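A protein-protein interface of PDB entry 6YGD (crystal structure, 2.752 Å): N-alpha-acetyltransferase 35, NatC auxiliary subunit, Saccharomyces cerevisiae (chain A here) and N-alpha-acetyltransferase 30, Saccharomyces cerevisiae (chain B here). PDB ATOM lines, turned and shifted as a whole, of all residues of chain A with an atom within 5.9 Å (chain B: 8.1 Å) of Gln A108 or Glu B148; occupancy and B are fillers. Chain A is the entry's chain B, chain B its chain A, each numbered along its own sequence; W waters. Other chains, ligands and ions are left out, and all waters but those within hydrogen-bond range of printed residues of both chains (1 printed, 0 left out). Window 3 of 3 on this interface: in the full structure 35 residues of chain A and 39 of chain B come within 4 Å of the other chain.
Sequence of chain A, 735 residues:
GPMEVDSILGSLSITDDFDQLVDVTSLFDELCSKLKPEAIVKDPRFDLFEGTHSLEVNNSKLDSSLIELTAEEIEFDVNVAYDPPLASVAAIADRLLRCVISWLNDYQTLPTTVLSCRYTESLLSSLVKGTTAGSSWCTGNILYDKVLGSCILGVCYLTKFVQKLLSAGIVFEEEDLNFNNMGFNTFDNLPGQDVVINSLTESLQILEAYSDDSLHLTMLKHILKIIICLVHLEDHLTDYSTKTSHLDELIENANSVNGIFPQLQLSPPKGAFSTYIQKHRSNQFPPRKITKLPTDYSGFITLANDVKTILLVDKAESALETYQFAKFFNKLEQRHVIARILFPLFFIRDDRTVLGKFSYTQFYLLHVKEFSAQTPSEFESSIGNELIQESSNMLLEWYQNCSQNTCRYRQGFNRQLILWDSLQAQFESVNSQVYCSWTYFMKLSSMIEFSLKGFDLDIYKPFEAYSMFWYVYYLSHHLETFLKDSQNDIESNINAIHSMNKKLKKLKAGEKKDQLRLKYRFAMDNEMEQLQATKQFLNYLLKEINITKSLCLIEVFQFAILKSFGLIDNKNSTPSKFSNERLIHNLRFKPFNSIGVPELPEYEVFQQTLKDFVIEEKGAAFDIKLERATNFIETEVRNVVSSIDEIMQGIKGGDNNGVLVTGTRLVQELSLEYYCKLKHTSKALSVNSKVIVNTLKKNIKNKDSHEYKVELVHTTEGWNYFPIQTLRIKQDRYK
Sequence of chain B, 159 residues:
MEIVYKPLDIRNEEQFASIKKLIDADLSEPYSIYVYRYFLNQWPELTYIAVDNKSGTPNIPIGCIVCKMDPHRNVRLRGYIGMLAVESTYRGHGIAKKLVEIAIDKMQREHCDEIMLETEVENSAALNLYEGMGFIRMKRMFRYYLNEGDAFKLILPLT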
ATOM      1  N   SER A 102     -14.218  16.719 -36.384  1.00  0.00           N
ATOM      2  CA  SER A 102     -14.670  16.937 -35.015  1.00  0.00           C
ATOM      3  C   SER A 102     -13.524  17.396 -34.126  1.00  0.00           C
ATOM      4  O   SER A 102     -13.723  18.232 -33.238  1.00  0.00           O
ATOM      5  CB  SER A 102     -15.306  15.661 -34.461  1.00  0.00           C
ATOM      6  OG  SER A 102     -15.927  15.905 -33.211  1.00  0.00           O
ATOM      7  N   TRP A 103     -12.314  16.894 -34.378  1.00  0.00           N
ATOM      8  CA  TRP A 103     -11.160  17.256 -33.559  1.00  0.00           C
ATOM      9  C   TRP A 103     -10.726  18.698 -33.806  1.00  0.00           C
ATOM     10  O   TRP A 103     -10.487  19.452 -32.855  1.00  0.00           O
ATOM     11  CB  TRP A 103     -10.017  16.281 -33.837  1.00  0.00           C
ATOM     12  CG  TRP A 103      -8.675  16.675 -33.295  1.00  0.00           C
ATOM     13  CD1 TRP A 103      -8.395  17.147 -32.046  1.00  0.00           C
ATOM     14  CD2 TRP A 103      -7.421  16.583 -33.979  1.00  0.00           C
ATOM     15  NE1 TRP A 103      -7.044  17.373 -31.918  1.00  0.00           N
ATOM     16  CE2 TRP A 103      -6.425  17.034 -33.093  1.00  0.00           C
ATOM     17  CE3 TRP A 103      -7.045  16.170 -35.262  1.00  0.00           C
ATOM     18  CZ2 TRP A 103      -5.077  17.084 -33.447  1.00  0.00           C
ATOM     19  CZ3 TRP A 103      -5.708  16.222 -35.611  1.00  0.00           C
ATOM     20  CH2 TRP A 103      -4.741  16.674 -34.708  1.00  0.00           C
ATOM     21  N   LEU A 104     -10.632  19.104 -35.073  1.00  0.00           N
ATOM     22  CA  LEU A 104     -10.133  20.428 -35.427  1.00  0.00           C
ATOM     23  C   LEU A 104     -11.249  21.465 -35.517  1.00  0.00           C
ATOM     24  O   LEU A 104     -11.178  22.513 -34.869  1.00  0.00           O
ATOM     25  CB  LEU A 104      -9.369  20.359 -36.753  1.00  0.00           C
ATOM     26  CG  LEU A 104      -8.203  19.368 -36.819  1.00  0.00           C
ATOM     27  CD1 LEU A 104      -7.606  19.319 -38.219  1.00  0.00           C
ATOM     28  CD2 LEU A 104      -7.140  19.722 -35.802  1.00  0.00           C
ATOM     29  N   ASN A 105     -12.285  21.186 -36.312  1.00  0.00           N
ATOM     30  CA  ASN A 105     -13.355  22.160 -36.509  1.00  0.00           C
ATOM     31  C   ASN A 105     -14.214  22.311 -35.260  1.00  0.00           C
ATOM     32  O   ASN A 105     -14.561  23.433 -34.875  1.00  0.00           O
ATOM     33  CB  ASN A 105     -14.220  21.759 -37.704  1.00  0.00           C
ATOM     34  CG  ASN A 105     -13.473  21.833 -39.017  1.00  0.00           C
ATOM     35  OD1 ASN A 105     -12.525  21.081 -39.249  1.00  0.00           O
ATOM     36  ND2 ASN A 105     -13.898  22.741 -39.889  1.00  0.00           N
ATOM     37  N   ASP A 106     -14.574  21.202 -34.620  1.00  0.00           N
ATOM     38  CA  ASP A 106     -15.441  21.224 -33.449  1.00  0.00           C
ATOM     39  C   ASP A 106     -14.665  21.302 -32.140  1.00  0.00           C
ATOM     40  O   ASP A 106     -15.274  21.207 -31.068  1.00  0.00           O
ATOM     41  CB  ASP A 106     -16.352  19.993 -33.447  1.00  0.00           C
ATOM     42  CG  ASP A 106     -17.361  20.016 -34.577  1.00  0.00           C
ATOM     43  OD1 ASP A 106     -17.396  21.017 -35.321  1.00  0.00           O
ATOM     44  OD2 ASP A 106     -18.119  19.032 -34.722  1.00  0.00           O
ATOM     45  N   TYR A 107     -13.340  21.456 -32.208  1.00  0.00           N
ATOM     46  CA  TYR A 107     -12.484  21.664 -31.036  1.00  0.00           C
ATOM     47  C   TYR A 107     -12.569  20.505 -30.044  1.00  0.00           C
ATOM     48  O   TYR A 107     -12.353  20.687 -28.843  1.00  0.00           O
ATOM     49  CB  TYR A 107     -12.812  22.987 -30.335  1.00  0.00           C
ATOM     50  CG  TYR A 107     -12.739  24.202 -31.236  1.00  0.00           C
ATOM     51  CD1 TYR A 107     -11.529  24.831 -31.491  1.00  0.00           C
ATOM     52  CD2 TYR A 107     -13.884  24.723 -31.827  1.00  0.00           C
ATOM     53  CE1 TYR A 107     -11.457  25.941 -32.315  1.00  0.00           C
ATOM     54  CE2 TYR A 107     -13.821  25.830 -32.651  1.00  0.00           C
ATOM     55  CZ  TYR A 107     -12.605  26.436 -32.892  1.00  0.00           C
ATOM     56  OH  TYR A 107     -12.537  27.543 -33.710  1.00  0.00           O
ATOM     57  N   GLN A 108     -12.878  19.306 -30.527  1.00  0.00           N
ATOM     58  CA  GLN A 108     -12.954  18.148 -29.654  1.00  0.00           C
ATOM     59  C   GLN A 108     -11.556  17.637 -29.317  1.00  0.00           C
ATOM     60  O   GLN A 108     -10.551  18.042 -29.909  1.00  0.00           O
ATOM     61  CB  GLN A 108     -13.790  17.041 -30.294  1.00  0.00           C
ATOM     62  CG  GLN A 108     -15.237  17.430 -30.515  1.00  0.00           C
ATOM     63  CD  GLN A 108     -15.905  17.908 -29.245  1.00  0.00           C
ATOM     64  OE1 GLN A 108     -15.721  17.325 -28.179  1.00  0.00           O
ATOM     65  NE2 GLN A 108     -16.679  18.981 -29.352  1.00  0.00           N
ATOM     66  N   THR A 109     -11.501  16.732 -28.346  1.00  0.00           N
ATOM     67  CA  THR A 109     -10.229  16.216 -27.867  1.00  0.00           C
ATOM     68  C   THR A 109      -9.666  15.165 -28.817  1.00  0.00           C
ATOM     69  O   THR A 109     -10.404  14.430 -29.481  1.00  0.00           O
ATOM     70  CB  THR A 109     -10.380  15.612 -26.472  1.00  0.00           C
ATOM     71  OG1 THR A 109     -11.198  14.439 -26.547  1.00  0.00           O
ATOM     72  CG2 THR A 109     -11.025  16.610 -25.531  1.00  0.00           C
ATOM     73  N   LEU A 110      -8.337  15.102 -28.867  1.00  0.00           N
ATOM     74  CA  LEU A 110      -7.659  14.123 -29.713  1.00  0.00           C
ATOM     75  C   LEU A 110      -7.957  12.680 -29.321  1.00  0.00           C
ATOM     76  O   LEU A 110      -8.218  11.863 -30.222  1.00  0.00           O
ATOM     77  CB  LEU A 110      -6.153  14.413 -29.702  1.00  0.00           C
ATOM     78  CG  LEU A 110      -5.251  13.642 -30.664  1.00  0.00           C
ATOM     79  CD1 LEU A 110      -5.740  13.809 -32.087  1.00  0.00           C
ATOM     80  CD2 LEU A 110      -3.817  14.118 -30.530  1.00  0.00           C
ATOM     81  N   THR A 112     -10.604  11.299 -28.053  1.00  0.00           N
ATOM     82  CA  THR A 112     -11.972  10.928 -28.387  1.00  0.00           C
ATOM     83  C   THR A 112     -12.295  11.129 -29.861  1.00  0.00           C
ATOM     84  O   THR A 112     -13.467  11.051 -30.243  1.00  0.00           O
ATOM     85  CB  THR A 112     -12.963  11.722 -27.532  1.00  0.00           C
ATOM     86  OG1 THR A 112     -12.909  13.105 -27.900  1.00  0.00           O
ATOM     87  CG2 THR A 112     -12.627  11.580 -26.056  1.00  0.00           C
ATOM     88  N   THR A 113     -11.290  11.383 -30.696  1.00  0.00           N
ATOM     89  CA  THR A 113     -11.542  11.616 -32.112  1.00  0.00           C
ATOM     90  C   THR A 113     -10.616  10.775 -32.981  1.00  0.00           C
ATOM     91  O   THR A 113     -11.018   9.720 -33.485  1.00  0.00           O
ATOM     92  CB  THR A 113     -11.381  13.099 -32.450  1.00  0.00           C
ATOM     93  OG1 THR A 113     -10.160  13.591 -31.885  1.00  0.00           O
ATOM     94  CG2 THR A 113     -12.555  13.899 -31.900  1.00  0.00           C
ATOM     95  N   LEU A 177      -7.077  24.343 -29.822  1.00  0.00           N
ATOM     96  CA  LEU A 177      -6.755  23.051 -30.403  1.00  0.00           C
ATOM     97  C   LEU A 177      -6.220  22.128 -29.321  1.00  0.00           C
ATOM     98  O   LEU A 177      -5.318  22.501 -28.566  1.00  0.00           O
ATOM     99  CB  LEU A 177      -5.732  23.202 -31.530  1.00  0.00           C
ATOM    100  CG  LEU A 177      -5.252  21.928 -32.218  1.00  0.00           C
ATOM    101  CD1 LEU A 177      -6.418  21.019 -32.546  1.00  0.00           C
ATOM    102  CD2 LEU A 177      -4.511  22.313 -33.481  1.00  0.00           C
ATOM    103  N   ASN A 178      -6.772  20.923 -29.258  1.00  0.00           N
ATOM    104  CA  ASN A 178      -6.357  19.930 -28.279  1.00  0.00           C
ATOM    105  C   ASN A 178      -5.400  18.936 -28.918  1.00  0.00           C
ATOM    106  O   ASN A 178      -5.703  18.358 -29.966  1.00  0.00           O
ATOM    107  CB  ASN A 178      -7.558  19.190 -27.693  1.00  0.00           C
ATOM    108  CG  ASN A 178      -7.145  18.039 -26.792  1.00  0.00           C
ATOM    109  OD1 ASN A 178      -7.268  16.869 -27.158  1.00  0.00           O
ATOM    110  ND2 ASN A 178      -6.634  18.368 -25.612  1.00  0.00           N
ATOM    111  N   ARG A 288     -13.761  10.584 -21.065  1.00  0.00           N
ATOM    112  CA  ARG A 288     -14.565  11.507 -21.850  1.00  0.00           C
ATOM    113  C   ARG A 288     -15.373  10.730 -22.877  1.00  0.00           C
ATOM    114  O   ARG A 288     -14.836   9.858 -23.566  1.00  0.00           O
ATOM    115  CB  ARG A 288     -13.680  12.545 -22.548  1.00  0.00           C
ATOM    116  CG  ARG A 288     -14.432  13.738 -23.100  1.00  0.00           C
ATOM    117  CD  ARG A 288     -13.467  14.821 -23.543  1.00  0.00           C
ATOM    118  NE  ARG A 288     -14.160  16.027 -23.987  1.00  0.00           N
ATOM    119  CZ  ARG A 288     -14.563  16.238 -25.236  1.00  0.00           C
ATOM    120  NH1 ARG A 288     -14.346  15.321 -26.170  1.00  0.00           N
ATOM    121  NH2 ARG A 288     -15.185  17.366 -25.551  1.00  0.00           N
ATOM    122  N   THR A 291     -18.098  12.846 -28.625  1.00  0.00           N
ATOM    123  CA  THR A 291     -19.121  13.766 -29.097  1.00  0.00           C
ATOM    124  C   THR A 291     -19.575  13.384 -30.502  1.00  0.00           C
ATOM    125  O   THR A 291     -18.811  12.831 -31.298  1.00  0.00           O
ATOM    126  CB  THR A 291     -18.591  15.201 -29.078  1.00  0.00           C
ATOM    127  OG1 THR A 291     -17.983  15.465 -27.807  1.00  0.00           O
ATOM    128  CG2 THR A 291     -19.719  16.201 -29.297  1.00  0.00           C
ATOM    129  N   SER B  28     -20.632  20.336 -12.737  1.00  0.00           N
ATOM    130  CA  SER B  28     -20.200  19.510 -13.856  1.00  0.00           C
ATOM    131  C   SER B  28     -18.713  19.191 -13.814  1.00  0.00           C
ATOM    132  O   SER B  28     -18.317  18.076 -14.168  1.00  0.00           O
ATOM    133  CB  SER B  28     -20.539  20.190 -15.186  1.00  0.00           C
ATOM    134  OG  SER B  28     -19.919  21.459 -15.295  1.00  0.00           O
ATOM    135  N   GLU B  29     -17.878  20.142 -13.411  1.00  0.00           N
ATOM    136  CA  GLU B  29     -16.447  19.872 -13.314  1.00  0.00           C
ATOM    137  C   GLU B  29     -16.198  18.870 -12.187  1.00  0.00           C
ATOM    138  O   GLU B  29     -16.682  19.075 -11.065  1.00  0.00           O
ATOM    139  CB  GLU B  29     -15.673  21.162 -13.044  1.00  0.00           C
ATOM    140  CG  GLU B  29     -15.770  22.210 -14.135  1.00  0.00           C
ATOM    141  CD  GLU B  29     -15.128  21.774 -15.434  1.00  0.00           C
ATOM    142  OE1 GLU B  29     -15.862  21.702 -16.442  1.00  0.00           O
ATOM    143  OE2 GLU B  29     -13.904  21.502 -15.445  1.00  0.00           O
ATOM    144  N   GLU B 120     -20.171  29.763 -15.787  1.00  0.00           N
ATOM    145  CA  GLU B 120     -20.534  29.559 -17.182  1.00  0.00           C
ATOM    146  C   GLU B 120     -21.378  30.723 -17.678  1.00  0.00           C
ATOM    147  O   GLU B 120     -22.218  31.257 -16.948  1.00  0.00           O
ATOM    148  CB  GLU B 120     -21.300  28.246 -17.338  1.00  0.00           C
ATOM    149  CG  GLU B 120     -20.502  27.029 -16.914  1.00  0.00           C
ATOM    150  CD  GLU B 120     -21.376  25.899 -16.418  1.00  0.00           C
ATOM    151  OE1 GLU B 120     -21.800  25.951 -15.244  1.00  0.00           O
ATOM    152  OE2 GLU B 120     -21.639  24.968 -17.205  1.00  0.00           O
ATOM    153  N   MET B 141     -13.658  33.527 -21.125  1.00  0.00           N
ATOM    154  CA  MET B 141     -12.707  32.468 -21.436  1.00  0.00           C
ATOM    155  C   MET B 141     -13.318  31.492 -22.426  1.00  0.00           C
ATOM    156  O   MET B 141     -14.366  30.895 -22.154  1.00  0.00           O
ATOM    157  CB  MET B 141     -12.263  31.731 -20.169  1.00  0.00           C
ATOM    158  CG  MET B 141     -11.534  32.610 -19.170  1.00  0.00           C
ATOM    159  SD  MET B 141     -12.652  33.628 -18.191  1.00  0.00           S
ATOM    160  CE  MET B 141     -12.930  32.564 -16.775  1.00  0.00           C
ATOM    161  N   PHE B 142     -12.645  31.326 -23.559  1.00  0.00           N
ATOM    162  CA  PHE B 142     -13.110  30.467 -24.643  1.00  0.00           C
ATOM    163  C   PHE B 142     -13.053  28.999 -24.218  1.00  0.00           C
ATOM    164  O   PHE B 142     -11.966  28.456 -23.992  1.00  0.00           O
ATOM    165  CB  PHE B 142     -12.256  30.720 -25.880  1.00  0.00           C
ATOM    166  CG  PHE B 142     -12.756  30.044 -27.120  1.00  0.00           C
ATOM    167  CD1 PHE B 142     -13.982  30.386 -27.663  1.00  0.00           C
ATOM    168  CD2 PHE B 142     -11.988  29.083 -27.755  1.00  0.00           C
ATOM    169  CE1 PHE B 142     -14.441  29.773 -28.811  1.00  0.00           C
ATOM    170  CE2 PHE B 142     -12.439  28.465 -28.905  1.00  0.00           C
ATOM    171  CZ  PHE B 142     -13.669  28.809 -29.434  1.00  0.00           C
ATOM    172  N   ARG B 143     -14.226  28.362 -24.111  1.00  0.00           N
ATOM    173  CA  ARG B 143     -14.359  26.927 -23.822  1.00  0.00           C
ATOM    174  C   ARG B 143     -13.596  26.532 -22.555  1.00  0.00           C
ATOM    175  O   ARG B 143     -12.837  25.560 -22.528  1.00  0.00           O
ATOM    176  CB  ARG B 143     -13.913  26.088 -25.022  1.00  0.00           C
ATOM    177  CG  ARG B 143     -14.697  26.381 -26.295  1.00  0.00           C
ATOM    178  CD  ARG B 143     -14.064  25.751 -27.525  1.00  0.00           C
ATOM    179  NE  ARG B 143     -14.008  24.296 -27.441  1.00  0.00           N
ATOM    180  CZ  ARG B 143     -15.008  23.492 -27.786  1.00  0.00           C
ATOM    181  NH1 ARG B 143     -16.146  24.003 -28.236  1.00  0.00           N
ATOM    182  NH2 ARG B 143     -14.870  22.178 -27.682  1.00  0.00           N
ATOM    183  N   TYR B 144     -13.841  27.295 -21.486  1.00  0.00           N
ATOM    184  CA  TYR B 144     -13.059  27.190 -20.257  1.00  0.00           C
ATOM    185  C   TYR B 144     -13.304  25.872 -19.537  1.00  0.00           C
ATOM    186  O   TYR B 144     -12.395  25.331 -18.893  1.00  0.00           O
ATOM    187  CB  TYR B 144     -13.421  28.362 -19.348  1.00  0.00           C
ATOM    188  CG  TYR B 144     -12.651  28.476 -18.055  1.00  0.00           C
ATOM    189  CD1 TYR B 144     -11.341  28.926 -18.048  1.00  0.00           C
ATOM    190  CD2 TYR B 144     -13.252  28.190 -16.835  1.00  0.00           C
ATOM    191  CE1 TYR B 144     -10.638  29.052 -16.873  1.00  0.00           C
ATOM    192  CE2 TYR B 144     -12.552  28.314 -15.652  1.00  0.00           C
ATOM    193  CZ  TYR B 144     -11.246  28.749 -15.677  1.00  0.00           C
ATOM    194  OH  TYR B 144     -10.535  28.878 -14.507  1.00  0.00           O
ATOM    195  N   TYR B 145     -14.518  25.346 -19.641  1.00  0.00           N
ATOM    196  CA  TYR B 145     -14.971  24.207 -18.864  1.00  0.00           C
ATOM    197  C   TYR B 145     -14.928  22.920 -19.680  1.00  0.00           C
ATOM    198  O   TYR B 145     -14.875  22.925 -20.915  1.00  0.00           O
ATOM    199  CB  TYR B 145     -16.384  24.464 -18.343  1.00  0.00           C
ATOM    200  CG  TYR B 145     -16.400  25.456 -17.212  1.00  0.00           C
ATOM    201  CD1 TYR B 145     -15.916  25.099 -15.963  1.00  0.00           C
ATOM    202  CD2 TYR B 145     -16.884  26.746 -17.387  1.00  0.00           C
ATOM    203  CE1 TYR B 145     -15.925  25.989 -14.917  1.00  0.00           C
ATOM    204  CE2 TYR B 145     -16.896  27.650 -16.341  1.00  0.00           C
ATOM    205  CZ  TYR B 145     -16.409  27.266 -15.109  1.00  0.00           C
ATOM    206  OH  TYR B 145     -16.405  28.143 -14.051  1.00  0.00           O
ATOM    207  N   LEU B 146     -14.964  21.802 -18.941  1.00  0.00           N
ATOM    208  CA  LEU B 146     -14.912  20.464 -19.522  1.00  0.00           C
ATOM    209  C   LEU B 146     -16.061  20.222 -20.490  1.00  0.00           C
ATOM    210  O   LEU B 146     -15.903  19.466 -21.454  1.00  0.00           O
ATOM    211  CB  LEU B 146     -14.940  19.415 -18.405  1.00  0.00           C
ATOM    212  CG  LEU B 146     -14.065  18.171 -18.545  1.00  0.00           C
ATOM    213  CD1 LEU B 146     -12.602  18.566 -18.422  1.00  0.00           C
ATOM    214  CD2 LEU B 146     -14.437  17.115 -17.503  1.00  0.00           C
ATOM    215  N   ASN B 147     -17.221  20.840 -20.246  1.00  0.00           N
ATOM    216  CA  ASN B 147     -18.373  20.725 -21.129  1.00  0.00           C
ATOM    217  C   ASN B 147     -18.280  21.647 -22.338  1.00  0.00           C
ATOM    218  O   ASN B 147     -19.273  21.809 -23.059  1.00  0.00           O
ATOM    219  CB  ASN B 147     -19.668  20.990 -20.351  1.00  0.00           C
ATOM    220  CG  ASN B 147     -19.662  22.314 -19.610  1.00  0.00           C
ATOM    221  OD1 ASN B 147     -19.569  23.377 -20.216  1.00  0.00           O
ATOM    222  ND2 ASN B 147     -19.803  22.255 -18.292  1.00  0.00           N
ATOM    223  N   GLU B 148     -17.109  22.250 -22.564  1.00  0.00           N
ATOM    224  CA  GLU B 148     -16.782  23.092 -23.713  1.00  0.00           C
ATOM    225  C   GLU B 148     -17.523  24.429 -23.718  1.00  0.00           C
ATOM    226  O   GLU B 148     -17.561  25.108 -24.752  1.00  0.00           O
ATOM    227  CB  GLU B 148     -17.035  22.351 -25.034  1.00  0.00           C
ATOM    228  CG  GLU B 148     -16.397  20.968 -25.097  1.00  0.00           C
ATOM    229  CD  GLU B 148     -17.290  19.933 -25.770  1.00  0.00           C
ATOM    230  OE1 GLU B 148     -18.221  20.332 -26.503  1.00  0.00           O
ATOM    231  OE2 GLU B 148     -17.066  18.719 -25.564  1.00  0.00           O
ATOM    232  N   GLY B 149     -18.101  24.838 -22.591  1.00  0.00           N
ATOM    233  CA  GLY B 149     -18.796  26.110 -22.517  1.00  0.00           C
ATOM    234  C   GLY B 149     -17.868  27.245 -22.118  1.00  0.00           C
ATOM    235  O   GLY B 149     -16.890  27.048 -21.402  1.00  0.00           O
ATOM    236  N   ASP B 150     -18.179  28.447 -22.598  1.00  0.00           N
ATOM    237  CA  ASP B 150     -17.372  29.602 -22.236  1.00  0.00           C
ATOM    238  C   ASP B 150     -17.646  29.999 -20.788  1.00  0.00           C
ATOM    239  O   ASP B 150     -18.663  29.627 -20.198  1.00  0.00           O
ATOM    240  CB  ASP B 150     -17.648  30.776 -23.176  1.00  0.00           C
ATOM    241  CG  ASP B 150     -17.138  30.528 -24.582  1.00  0.00           C
ATOM    242  OD1 ASP B 150     -16.603  29.429 -24.842  1.00  0.00           O
ATOM    243  OD2 ASP B 150     -17.271  31.441 -25.425  1.00  0.00           O
ATOM    244  N   ALA B 151     -16.707  30.738 -20.198  1.00  0.00           N
ATOM    245  CA  ALA B 151     -16.843  31.187 -18.822  1.00  0.00           C
ATOM    246  C   ALA B 151     -16.678  32.696 -18.748  1.00  0.00           C
ATOM    247  O   ALA B 151     -15.971  33.301 -19.559  1.00  0.00           O
ATOM    248  CB  ALA B 151     -15.822  30.532 -17.898  1.00  0.00           C
HETATM  249  O   HOH W   1     -17.123  16.947 -22.964  1.00  0.00           O
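Gln A108 touches just one residue of chain B: Glu B148 (3.3 Å). Of chain A, only Gln A108 and Arg A288 come within 4 Å of Glu B148. Of the printed residues of chain B, Asp A106 touches Arg B143. Of the printed residues of chain B, Arg A288 touches Glu B148 (2.3 Å). Of the printed residues of chain B, Tyr A107 touches Arg B143 (3.1 Å). Of the printed residues of chain A, Arg B143 touches Asp A106 (3.5 Å) and Tyr A107 (3.1 Å). Tyr B144 touches none of the printed residues of chain A. Ser B28 touches none of the printed residues of chain A. The nearest residue of chain B that does not touch Gln A108 is Arg B143 (4.04 Å).
Among the printed residues, pairs that only touch across the chains: Asp A106 with Arg B143.
Water W1 lies within hydrogen-bond range of OE2 of Glu B148 (3.1 Å), O of Leu B146 (3.2 Å) and NH2 of Arg A288 (3.3 Å).
The guanidinium group (NH2) of Arg B143 is in hydrogen-bond range of the backbone carbonyl oxygen (O) of Tyr A107, 3.1 Å away. The side-chain carboxylate (OE2) of Glu B148 sits close to the side-chain amide oxygen (OE1) of Gln A108. NH2 of Arg A288 sits close to OE2 of Glu B148.
Of the 15 printed residues of chain A, 4 touch a printed residue of chain B. Of the 14 printed residues of chain B, 2 touch a printed residue of chain A. Among the printed residues, 4 pairs touch across the chains. Among the printed residues, Asp or Glu carboxylates within 4 Å of a Lys or Arg side-chain nitrogen of the other chain: Arg A288 with Glu B148.
The side-chain carboxylate (OD1) of Asp B150 is in hydrogen-bond range of the backbone NH (N) of Arg B143, 2.7 Å away. O of Ser A102 is in hydrogen-bond range of N of Tyr A107 (3.4 Å). The backbone carbonyl oxygen of Ser A102 lies within hydrogen-bond range of the backbone NH of Gln A108. The side-chain amide nitrogen (NE2) of Gln A108 is in hydrogen-bond range of the backbone carbonyl oxygen (O) of Asp A106. The side-chain amide oxygen (OE1) of Gln A108 is in hydrogen-bond range of the side-chain hydroxyl (OG1) of Thr A291, at 3.0 Å. NH1 of Arg A288 sits at hydrogen-bond distance from OG1 of Thr A112, 3.2 Å away.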
